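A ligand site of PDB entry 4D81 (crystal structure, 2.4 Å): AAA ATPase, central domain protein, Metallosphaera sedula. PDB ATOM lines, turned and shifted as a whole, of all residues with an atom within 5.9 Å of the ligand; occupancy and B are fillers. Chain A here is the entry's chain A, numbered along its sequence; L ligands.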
ATOM      1  N   GLU A  15       8.475   2.475  -8.131  1.00  0.00           N
ATOM      2  CA  GLU A  15       8.829   3.775  -8.683  1.00  0.00           C
ATOM      3  C   GLU A  15       9.872   4.475  -7.852  1.00  0.00           C
ATOM      4  O   GLU A  15      10.350   5.547  -8.221  1.00  0.00           O
ATOM      5  CB  GLU A  15       7.589   4.674  -8.714  1.00  0.00           C
ATOM      6  CG  GLU A  15       6.400   4.052  -9.435  1.00  0.00           C
ATOM      7  CD  GLU A  15       5.185   4.974  -9.533  1.00  0.00           C
ATOM      8  OE1 GLU A  15       5.330   6.223  -9.685  1.00  0.00           O
ATOM      9  OE2 GLU A  15       4.045   4.445  -9.462  1.00  0.00           O
ATOM     10  N   ILE A  16      10.199   3.905  -6.706  1.00  0.00           N
ATOM     11  CA  ILE A  16      11.172   4.477  -5.797  1.00  0.00           C
ATOM     12  C   ILE A  16      12.496   3.720  -5.964  1.00  0.00           C
ATOM     13  O   ILE A  16      12.518   2.504  -5.866  1.00  0.00           O
ATOM     14  CB  ILE A  16      10.652   4.404  -4.338  1.00  0.00           C
ATOM     15  CG1 ILE A  16       9.234   5.006  -4.293  1.00  0.00           C
ATOM     16  CG2 ILE A  16      11.619   5.094  -3.366  1.00  0.00           C
ATOM     17  CD1 ILE A  16       8.564   4.977  -2.923  1.00  0.00           C
ATOM     18  N   VAL A  17      13.578   4.453  -6.179  1.00  0.00           N
ATOM     19  CA  VAL A  17      14.839   3.866  -6.607  1.00  0.00           C
ATOM     20  C   VAL A  17      15.530   3.113  -5.486  1.00  0.00           C
ATOM     21  O   VAL A  17      15.887   1.919  -5.609  1.00  0.00           O
ATOM     22  CB  VAL A  17      15.785   4.938  -7.165  1.00  0.00           C
ATOM     23  CG1 VAL A  17      17.200   4.391  -7.294  1.00  0.00           C
ATOM     24  CG2 VAL A  17      15.294   5.424  -8.498  1.00  0.00           C
ATOM     25  N   GLY A  18      15.737   3.766  -4.369  1.00  0.00           N
ATOM     26  CA  GLY A  18      16.458   3.037  -3.325  1.00  0.00           C
ATOM     27  C   GLY A  18      15.571   2.442  -2.266  1.00  0.00           C
ATOM     28  O   GLY A  18      14.592   1.760  -2.537  1.00  0.00           O
ATOM     29  N   LEU A  19      16.008   2.669  -1.039  1.00  0.00           N
ATOM     30  CA  LEU A  19      15.217   2.562   0.158  1.00  0.00           C
ATOM     31  C   LEU A  19      14.627   1.190   0.283  1.00  0.00           C
ATOM     32  O   LEU A  19      13.523   1.023   0.762  1.00  0.00           O
ATOM     33  CB  LEU A  19      14.138   3.652   0.159  1.00  0.00           C
ATOM     34  CG  LEU A  19      14.511   5.038  -0.372  1.00  0.00           C
ATOM     35  CD1 LEU A  19      13.295   5.951  -0.332  1.00  0.00           C
ATOM     36  CD2 LEU A  19      15.649   5.687   0.411  1.00  0.00           C
ATOM     37  N   PRO A  53      16.800  14.753   5.434  1.00  0.00           N
ATOM     38  CA  PRO A  53      16.820  15.894   4.527  1.00  0.00           C
ATOM     39  C   PRO A  53      15.637  15.880   3.575  1.00  0.00           C
ATOM     40  O   PRO A  53      15.089  14.829   3.276  1.00  0.00           O
ATOM     41  CB  PRO A  53      18.136  15.719   3.750  1.00  0.00           C
ATOM     42  CG  PRO A  53      18.361  14.240   3.754  1.00  0.00           C
ATOM     43  CD  PRO A  53      17.915  13.831   5.149  1.00  0.00           C
ATOM     44  N   PRO A  54      15.259  17.062   3.093  1.00  0.00           N
ATOM     45  CA  PRO A  54      14.144  17.160   2.178  1.00  0.00           C
ATOM     46  C   PRO A  54      14.536  16.615   0.820  1.00  0.00           C
ATOM     47  O   PRO A  54      15.702  16.587   0.486  1.00  0.00           O
ATOM     48  CB  PRO A  54      13.882  18.660   2.106  1.00  0.00           C
ATOM     49  CG  PRO A  54      15.224  19.254   2.350  1.00  0.00           C
ATOM     50  CD  PRO A  54      15.792  18.393   3.446  1.00  0.00           C
ATOM     51  N   GLY A  55      13.559  16.202   0.056  1.00  0.00           N
ATOM     52  CA  GLY A  55      13.819  15.676  -1.253  1.00  0.00           C
ATOM     53  C   GLY A  55      14.493  14.332  -1.244  1.00  0.00           C
ATOM     54  O   GLY A  55      15.186  13.950  -2.208  1.00  0.00           O
ATOM     55  N   CYS A  56      14.284  13.587  -0.166  1.00  0.00           N
ATOM     56  CA  CYS A  56      14.901  12.262  -0.109  1.00  0.00           C
ATOM     57  C   CYS A  56      13.928  11.116  -0.227  1.00  0.00           C
ATOM     58  O   CYS A  56      14.354   9.971  -0.170  1.00  0.00           O
ATOM     59  CB  CYS A  56      15.790  12.165   1.102  1.00  0.00           C
ATOM     60  SG  CYS A  56      17.472  12.596   0.574  1.00  0.00           S
ATOM     61  N   GLY A  57      12.644  11.417  -0.468  1.00  0.00           N
ATOM     62  CA  GLY A  57      11.623  10.400  -0.732  1.00  0.00           C
ATOM     63  C   GLY A  57      10.674  10.092   0.422  1.00  0.00           C
ATOM     64  O   GLY A  57      10.043   9.040   0.445  1.00  0.00           O
ATOM     65  N   LYS A  58      10.574  10.977   1.399  1.00  0.00           N
ATOM     66  CA  LYS A  58       9.688  10.708   2.532  1.00  0.00           C
ATOM     67  C   LYS A  58       8.212  10.661   2.093  1.00  0.00           C
ATOM     68  O   LYS A  58       7.541   9.624   2.232  1.00  0.00           O
ATOM     69  CB  LYS A  58       9.956  11.687   3.666  1.00  0.00           C
ATOM     70  CG  LYS A  58      11.212  11.339   4.437  1.00  0.00           C
ATOM     71  CD  LYS A  58      11.472  12.296   5.590  1.00  0.00           C
ATOM     72  CE  LYS A  58      11.438  13.767   5.200  1.00  0.00           C
ATOM     73  NZ  LYS A  58      12.443  13.962   4.128  1.00  0.00           N
ATOM     74  N   THR A  59       7.729  11.751   1.505  1.00  0.00           N
ATOM     75  CA  THR A  59       6.388  11.766   0.958  1.00  0.00           C
ATOM     76  C   THR A  59       6.176  10.583   0.036  1.00  0.00           C
ATOM     77  O   THR A  59       5.314   9.749   0.232  1.00  0.00           O
ATOM     78  CB  THR A  59       6.129  13.087   0.219  1.00  0.00           C
ATOM     79  OG1 THR A  59       6.389  14.186   1.113  1.00  0.00           O
ATOM     80  CG2 THR A  59       4.668  13.154  -0.237  1.00  0.00           C
ATOM     81  N   MET A  60       7.019  10.489  -0.963  1.00  0.00           N
ATOM     82  CA  MET A  60       6.993   9.383  -1.904  1.00  0.00           C
ATOM     83  C   MET A  60       6.727   7.984  -1.275  1.00  0.00           C
ATOM     84  O   MET A  60       5.901   7.200  -1.721  1.00  0.00           O
ATOM     85  CB  MET A  60       8.347   9.400  -2.628  1.00  0.00           C
ATOM     86  CG  MET A  60       8.398   8.605  -3.915  1.00  0.00           C
ATOM     87  SD  MET A  60       9.553   9.330  -5.097  1.00  0.00           S
ATOM     88  CE  MET A  60       8.951   8.593  -6.607  1.00  0.00           C
ATOM     89  N   ILE A  61       7.480   7.669  -0.255  1.00  0.00           N
ATOM     90  CA  ILE A  61       7.399   6.332   0.307  1.00  0.00           C
ATOM     91  C   ILE A  61       6.105   6.125   1.140  1.00  0.00           C
ATOM     92  O   ILE A  61       5.501   5.055   1.087  1.00  0.00           O
ATOM     93  CB  ILE A  61       8.654   6.027   1.147  1.00  0.00           C
ATOM     94  CG1 ILE A  61       8.810   4.520   1.331  1.00  0.00           C
ATOM     95  CG2 ILE A  61       8.637   6.766   2.466  1.00  0.00           C
ATOM     96  CD1 ILE A  61       9.749   3.886   0.331  1.00  0.00           C
ATOM     97  N   PHE A 114      -0.872  10.702   6.387  1.00  0.00           N
ATOM     98  CA  PHE A 114       0.507  11.091   6.239  1.00  0.00           C
ATOM     99  C   PHE A 114       0.586  12.553   6.635  1.00  0.00           C
ATOM    100  O   PHE A 114      -0.069  13.367   6.045  1.00  0.00           O
ATOM    101  CB  PHE A 114       0.963  10.902   4.829  1.00  0.00           C
ATOM    102  CG  PHE A 114       2.281  11.537   4.546  1.00  0.00           C
ATOM    103  CD1 PHE A 114       3.427  11.048   5.127  1.00  0.00           C
ATOM    104  CD2 PHE A 114       2.367  12.629   3.701  1.00  0.00           C
ATOM    105  CE1 PHE A 114       4.643  11.625   4.856  1.00  0.00           C
ATOM    106  CE2 PHE A 114       3.584  13.226   3.441  1.00  0.00           C
ATOM    107  CZ  PHE A 114       4.727  12.728   4.021  1.00  0.00           C
ATOM    108  N   ASP A 116       2.986  15.661   6.876  1.00  0.00           N
ATOM    109  CA  ASP A 116       4.203  16.179   6.362  1.00  0.00           C
ATOM    110  C   ASP A 116       4.503  17.379   7.208  1.00  0.00           C
ATOM    111  O   ASP A 116       3.608  17.975   7.805  1.00  0.00           O
ATOM    112  CB  ASP A 116       3.989  16.564   4.892  1.00  0.00           C
ATOM    113  CG  ASP A 116       5.301  16.868   4.149  1.00  0.00           C
ATOM    114  OD1 ASP A 116       6.382  16.626   4.746  1.00  0.00           O
ATOM    115  OD2 ASP A 116       5.243  17.322   2.991  1.00  0.00           O
ATOM    116  N   ALA A 160       6.411  13.006   8.814  1.00  0.00           N
ATOM    117  CA  ALA A 160       7.689  13.344   8.190  1.00  0.00           C
ATOM    118  C   ALA A 160       8.157  14.705   8.609  1.00  0.00           C
ATOM    119  O   ALA A 160       7.363  15.675   8.735  1.00  0.00           O
ATOM    120  CB  ALA A 160       7.620  13.306   6.688  1.00  0.00           C
ATOM    121  N   ASN A 162      11.972  17.322   8.325  1.00  0.00           N
ATOM    122  CA  ASN A 162      13.393  17.457   8.033  1.00  0.00           C
ATOM    123  C   ASN A 162      14.068  18.300   9.096  1.00  0.00           C
ATOM    124  O   ASN A 162      15.197  18.741   8.927  1.00  0.00           O
ATOM    125  CB  ASN A 162      13.616  17.944   6.609  1.00  0.00           C
ATOM    126  CG  ASN A 162      12.859  19.205   6.320  1.00  0.00           C
ATOM    127  OD1 ASN A 162      13.032  20.198   7.027  1.00  0.00           O
ATOM    128  ND2 ASN A 162      12.002  19.174   5.282  1.00  0.00           N
ATOM    129  N   HIS A 188      23.604   4.771  -4.494  1.00  0.00           N
ATOM    130  CA  HIS A 188      22.212   5.202  -4.557  1.00  0.00           C
ATOM    131  C   HIS A 188      22.136   6.294  -5.660  1.00  0.00           C
ATOM    132  O   HIS A 188      21.323   6.206  -6.601  1.00  0.00           O
ATOM    133  CB  HIS A 188      21.736   5.716  -3.178  1.00  0.00           C
ATOM    134  CG  HIS A 188      20.249   5.905  -3.048  1.00  0.00           C
ATOM    135  ND1 HIS A 188      19.658   6.559  -1.983  1.00  0.00           N
ATOM    136  CD2 HIS A 188      19.228   5.522  -3.862  1.00  0.00           C
ATOM    137  CE1 HIS A 188      18.353   6.581  -2.137  1.00  0.00           C
ATOM    138  NE2 HIS A 188      18.060   5.965  -3.271  1.00  0.00           N
ATOM    139  N   LEU A 192      19.757   6.535  -9.052  1.00  0.00           N
ATOM    140  CA  LEU A 192      19.013   7.761  -9.344  1.00  0.00           C
ATOM    141  C   LEU A 192      19.483   8.377 -10.694  1.00  0.00           C
ATOM    142  O   LEU A 192      18.651   8.667 -11.597  1.00  0.00           O
ATOM    143  CB  LEU A 192      19.214   8.756  -8.192  1.00  0.00           C
ATOM    144  CG  LEU A 192      18.579   8.344  -6.850  1.00  0.00           C
ATOM    145  CD1 LEU A 192      19.110   9.173  -5.697  1.00  0.00           C
ATOM    146  CD2 LEU A 192      17.078   8.493  -6.925  1.00  0.00           C
ATOM    147  N   HIS A 195      18.390   6.209 -13.402  1.00  0.00           N
ATOM    148  CA  HIS A 195      16.943   6.321 -13.468  1.00  0.00           C
ATOM    149  C   HIS A 195      16.500   7.588 -14.198  1.00  0.00           C
ATOM    150  O   HIS A 195      15.868   7.539 -15.254  1.00  0.00           O
ATOM    151  CB  HIS A 195      16.362   6.272 -12.056  1.00  0.00           C
ATOM    152  CG  HIS A 195      14.880   6.459 -11.993  1.00  0.00           C
ATOM    153  ND1 HIS A 195      13.987   5.449 -12.264  1.00  0.00           N
ATOM    154  CD2 HIS A 195      14.125   7.551 -11.696  1.00  0.00           C
ATOM    155  CE1 HIS A 195      12.752   5.892 -12.131  1.00  0.00           C
ATOM    156  NE2 HIS A 195      12.808   7.170 -11.790  1.00  0.00           N
ATOM    157  N   TYR A 196      16.903   8.742 -13.674  1.00  0.00           N
ATOM    158  CA  TYR A 196      16.500   9.998 -14.334  1.00  0.00           C
ATOM    159  C   TYR A 196      17.082  10.195 -15.760  1.00  0.00           C
ATOM    160  O   TYR A 196      16.348  10.576 -16.689  1.00  0.00           O
ATOM    161  CB  TYR A 196      16.771  11.193 -13.401  1.00  0.00           C
ATOM    162  CG  TYR A 196      15.807  11.198 -12.274  1.00  0.00           C
ATOM    163  CD1 TYR A 196      14.451  11.280 -12.529  1.00  0.00           C
ATOM    164  CD2 TYR A 196      16.221  11.053 -10.971  1.00  0.00           C
ATOM    165  CE1 TYR A 196      13.518  11.241 -11.522  1.00  0.00           C
ATOM    166  CE2 TYR A 196      15.293  11.040  -9.938  1.00  0.00           C
ATOM    167  CZ  TYR A 196      13.928  11.131 -10.233  1.00  0.00           C
ATOM    168  OH  TYR A 196      12.961  11.128  -9.271  1.00  0.00           O
ATOM    169  N   ALA A 220      18.108  13.254  -3.745  1.00  0.00           N
ATOM    170  CA  ALA A 220      17.467  12.612  -4.885  1.00  0.00           C
ATOM    171  C   ALA A 220      16.724  13.574  -5.832  1.00  0.00           C
ATOM    172  O   ALA A 220      16.668  13.325  -7.055  1.00  0.00           O
ATOM    173  CB  ALA A 220      16.500  11.554  -4.386  1.00  0.00           C
ATOM    174  N   SER A 221      16.102  14.623  -5.271  1.00  0.00           N
ATOM    175  CA  SER A 221      15.434  15.616  -6.058  1.00  0.00           C
ATOM    176  C   SER A 221      16.480  16.541  -6.670  1.00  0.00           C
ATOM    177  O   SER A 221      16.303  16.903  -7.827  1.00  0.00           O
ATOM    178  CB  SER A 221      14.421  16.438  -5.269  1.00  0.00           C
ATOM    179  OG  SER A 221      15.001  16.969  -4.115  1.00  0.00           O
ATOM    180  N   ARG A 224      17.604  14.691  -9.727  1.00  0.00           N
ATOM    181  CA  ARG A 224      16.587  14.945 -10.750  1.00  0.00           C
ATOM    182  C   ARG A 224      16.745  16.367 -11.328  1.00  0.00           C
ATOM    183  O   ARG A 224      16.698  16.574 -12.533  1.00  0.00           O
ATOM    184  CB  ARG A 224      15.186  14.722 -10.177  1.00  0.00           C
ATOM    185  CG  ARG A 224      14.021  15.015 -11.114  1.00  0.00           C
ATOM    186  CD  ARG A 224      12.756  15.365 -10.335  1.00  0.00           C
ATOM    187  NE  ARG A 224      12.952  16.581  -9.550  1.00  0.00           N
ATOM    188  CZ  ARG A 224      12.162  16.986  -8.551  1.00  0.00           C
ATOM    189  NH1 ARG A 224      11.103  16.259  -8.206  1.00  0.00           N
ATOM    190  NH2 ARG A 224      12.433  18.114  -7.883  1.00  0.00           N
HETATM  191  P1  LIG L   1      10.684  14.317   0.994  1.00  0.00           P
HETATM  192  O1  LIG L   1       9.236  13.978   1.228  1.00  0.00           O
HETATM  193  O2  LIG L   1      11.040  15.762   1.264  1.00  0.00           O
HETATM  194  O3  LIG L   1      11.702  13.376   1.615  1.00  0.00           O
HETATM  195  P2  LIG L   1       9.715  13.624  -1.570  1.00  0.00           P
HETATM  196  O4  LIG L   1       8.757  14.770  -1.614  1.00  0.00           O
HETATM  197  O5  LIG L   1       9.124  12.236  -1.329  1.00  0.00           O
HETATM  198  O6  LIG L   1      10.903  14.051  -0.578  1.00  0.00           O
HETATM  199  O7  LIG L   1      10.592  13.582  -2.921  1.00  0.00           O
HETATM  200  C1  LIG L   1      10.806  14.762  -3.680  1.00  0.00           C
HETATM  201  C2  LIG L   1      10.945  14.309  -5.109  1.00  0.00           C
HETATM  202  O8  LIG L   1      12.243  13.730  -5.225  1.00  0.00           O
HETATM  203  C3  LIG L   1       9.921  13.291  -5.655  1.00  0.00           C
HETATM  204  O9  LIG L   1       8.933  13.871  -6.528  1.00  0.00           O
HETATM  205  C4  LIG L   1      10.789  12.437  -6.528  1.00  0.00           C
HETATM  206  O10 LIG L   1      10.783  13.056  -7.835  1.00  0.00           O
HETATM  207  C5  LIG L   1      12.198  12.555  -6.014  1.00  0.00           C
HETATM  208  N1  LIG L   1      12.690  11.404  -5.234  1.00  0.00           N
HETATM  209  C6  LIG L   1      13.068  11.438  -3.944  1.00  0.00           C
HETATM  210  N2  LIG L   1      13.510  10.220  -3.552  1.00  0.00           N
HETATM  211  C7  LIG L   1      13.459   9.408  -4.597  1.00  0.00           C
HETATM  212  C8  LIG L   1      13.780   8.009  -4.828  1.00  0.00           C
HETATM  213  N3  LIG L   1      14.257   7.249  -3.823  1.00  0.00           N
HETATM  214  N4  LIG L   1      13.543   7.506  -6.048  1.00  0.00           N
HETATM  215  C9  LIG L   1      13.059   8.269  -7.059  1.00  0.00           C
HETATM  216  N5  LIG L   1      12.788   9.583  -6.923  1.00  0.00           N
HETATM  217  C10 LIG L   1      12.941  10.197  -5.721  1.00  0.00           C
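The backbone carbonyl oxygen (O) of Pro 53 is in hydrogen-bond range of the side-chain amino group (NZ) of Lys 58. O of Gly 55 is in hydrogen-bond range of N of Ala 220 (3.4 Å). O of Gly 55 is in hydrogen-bond range of N of Ser 221 (3.3 Å). N of Gly 18 sits close to NE2 of His 188.
The backbone NH of Lys 58 is in hydrogen-bond range of an oxygen (O3) of the ligand. An oxygen (O3) of the ligand is in salt-bridge range of the side-chain amino group (NZ) of Lys 58, at 2.7 Å. An oxygen (O1) of the ligand sits at hydrogen-bond distance from the backbone NH (N) of Thr 59 (2.7 Å). The side-chain hydroxyl of Thr 59 lies within hydrogen-bond range of an oxygen (O1) of the ligand (2.9 Å). The backbone NH of Met 60 sits at hydrogen-bond distance from an oxygen (O5) of the ligand (2.8 Å). A nitrogen (N5) of the ligand is in hydrogen-bond range of the side-chain hydroxyl (OH) of Tyr 196 (2.8 Å). The backbone NH (N) of Gly 55 lies within hydrogen-bond range of an oxygen (O2) of the ligand. The backbone NH (N) of Gly 57 is in hydrogen-bond range of an oxygen (O3) of the ligand (3.0 Å). The backbone NH (N) of Val 17 is in hydrogen-bond range of a nitrogen (N4) of the ligand, 3.1 Å away. An oxygen (O3) of the ligand is in hydrogen-bond range of the backbone NH (N) of Cys 56, 3.1 Å away. NH1 of Arg 224 is in hydrogen-bond range of O10 of the ligand (3.2 Å).
Merely in contact with the ligand: Ile 16, Gly 18, Leu 19, Pro 54, Leu 192, Ala 220 and Ser 221. Hydrophobic or aromatic side chains that line the ligand: Ile 16, Val 17, Leu 19, Met 60, Leu 192, Tyr 196 and Ala 220. Of the 25 residues printed, 16 come within 4 Å of the ligand. The nearest printed residue that does not touch the ligand is Glu 15 (4.01 Å).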
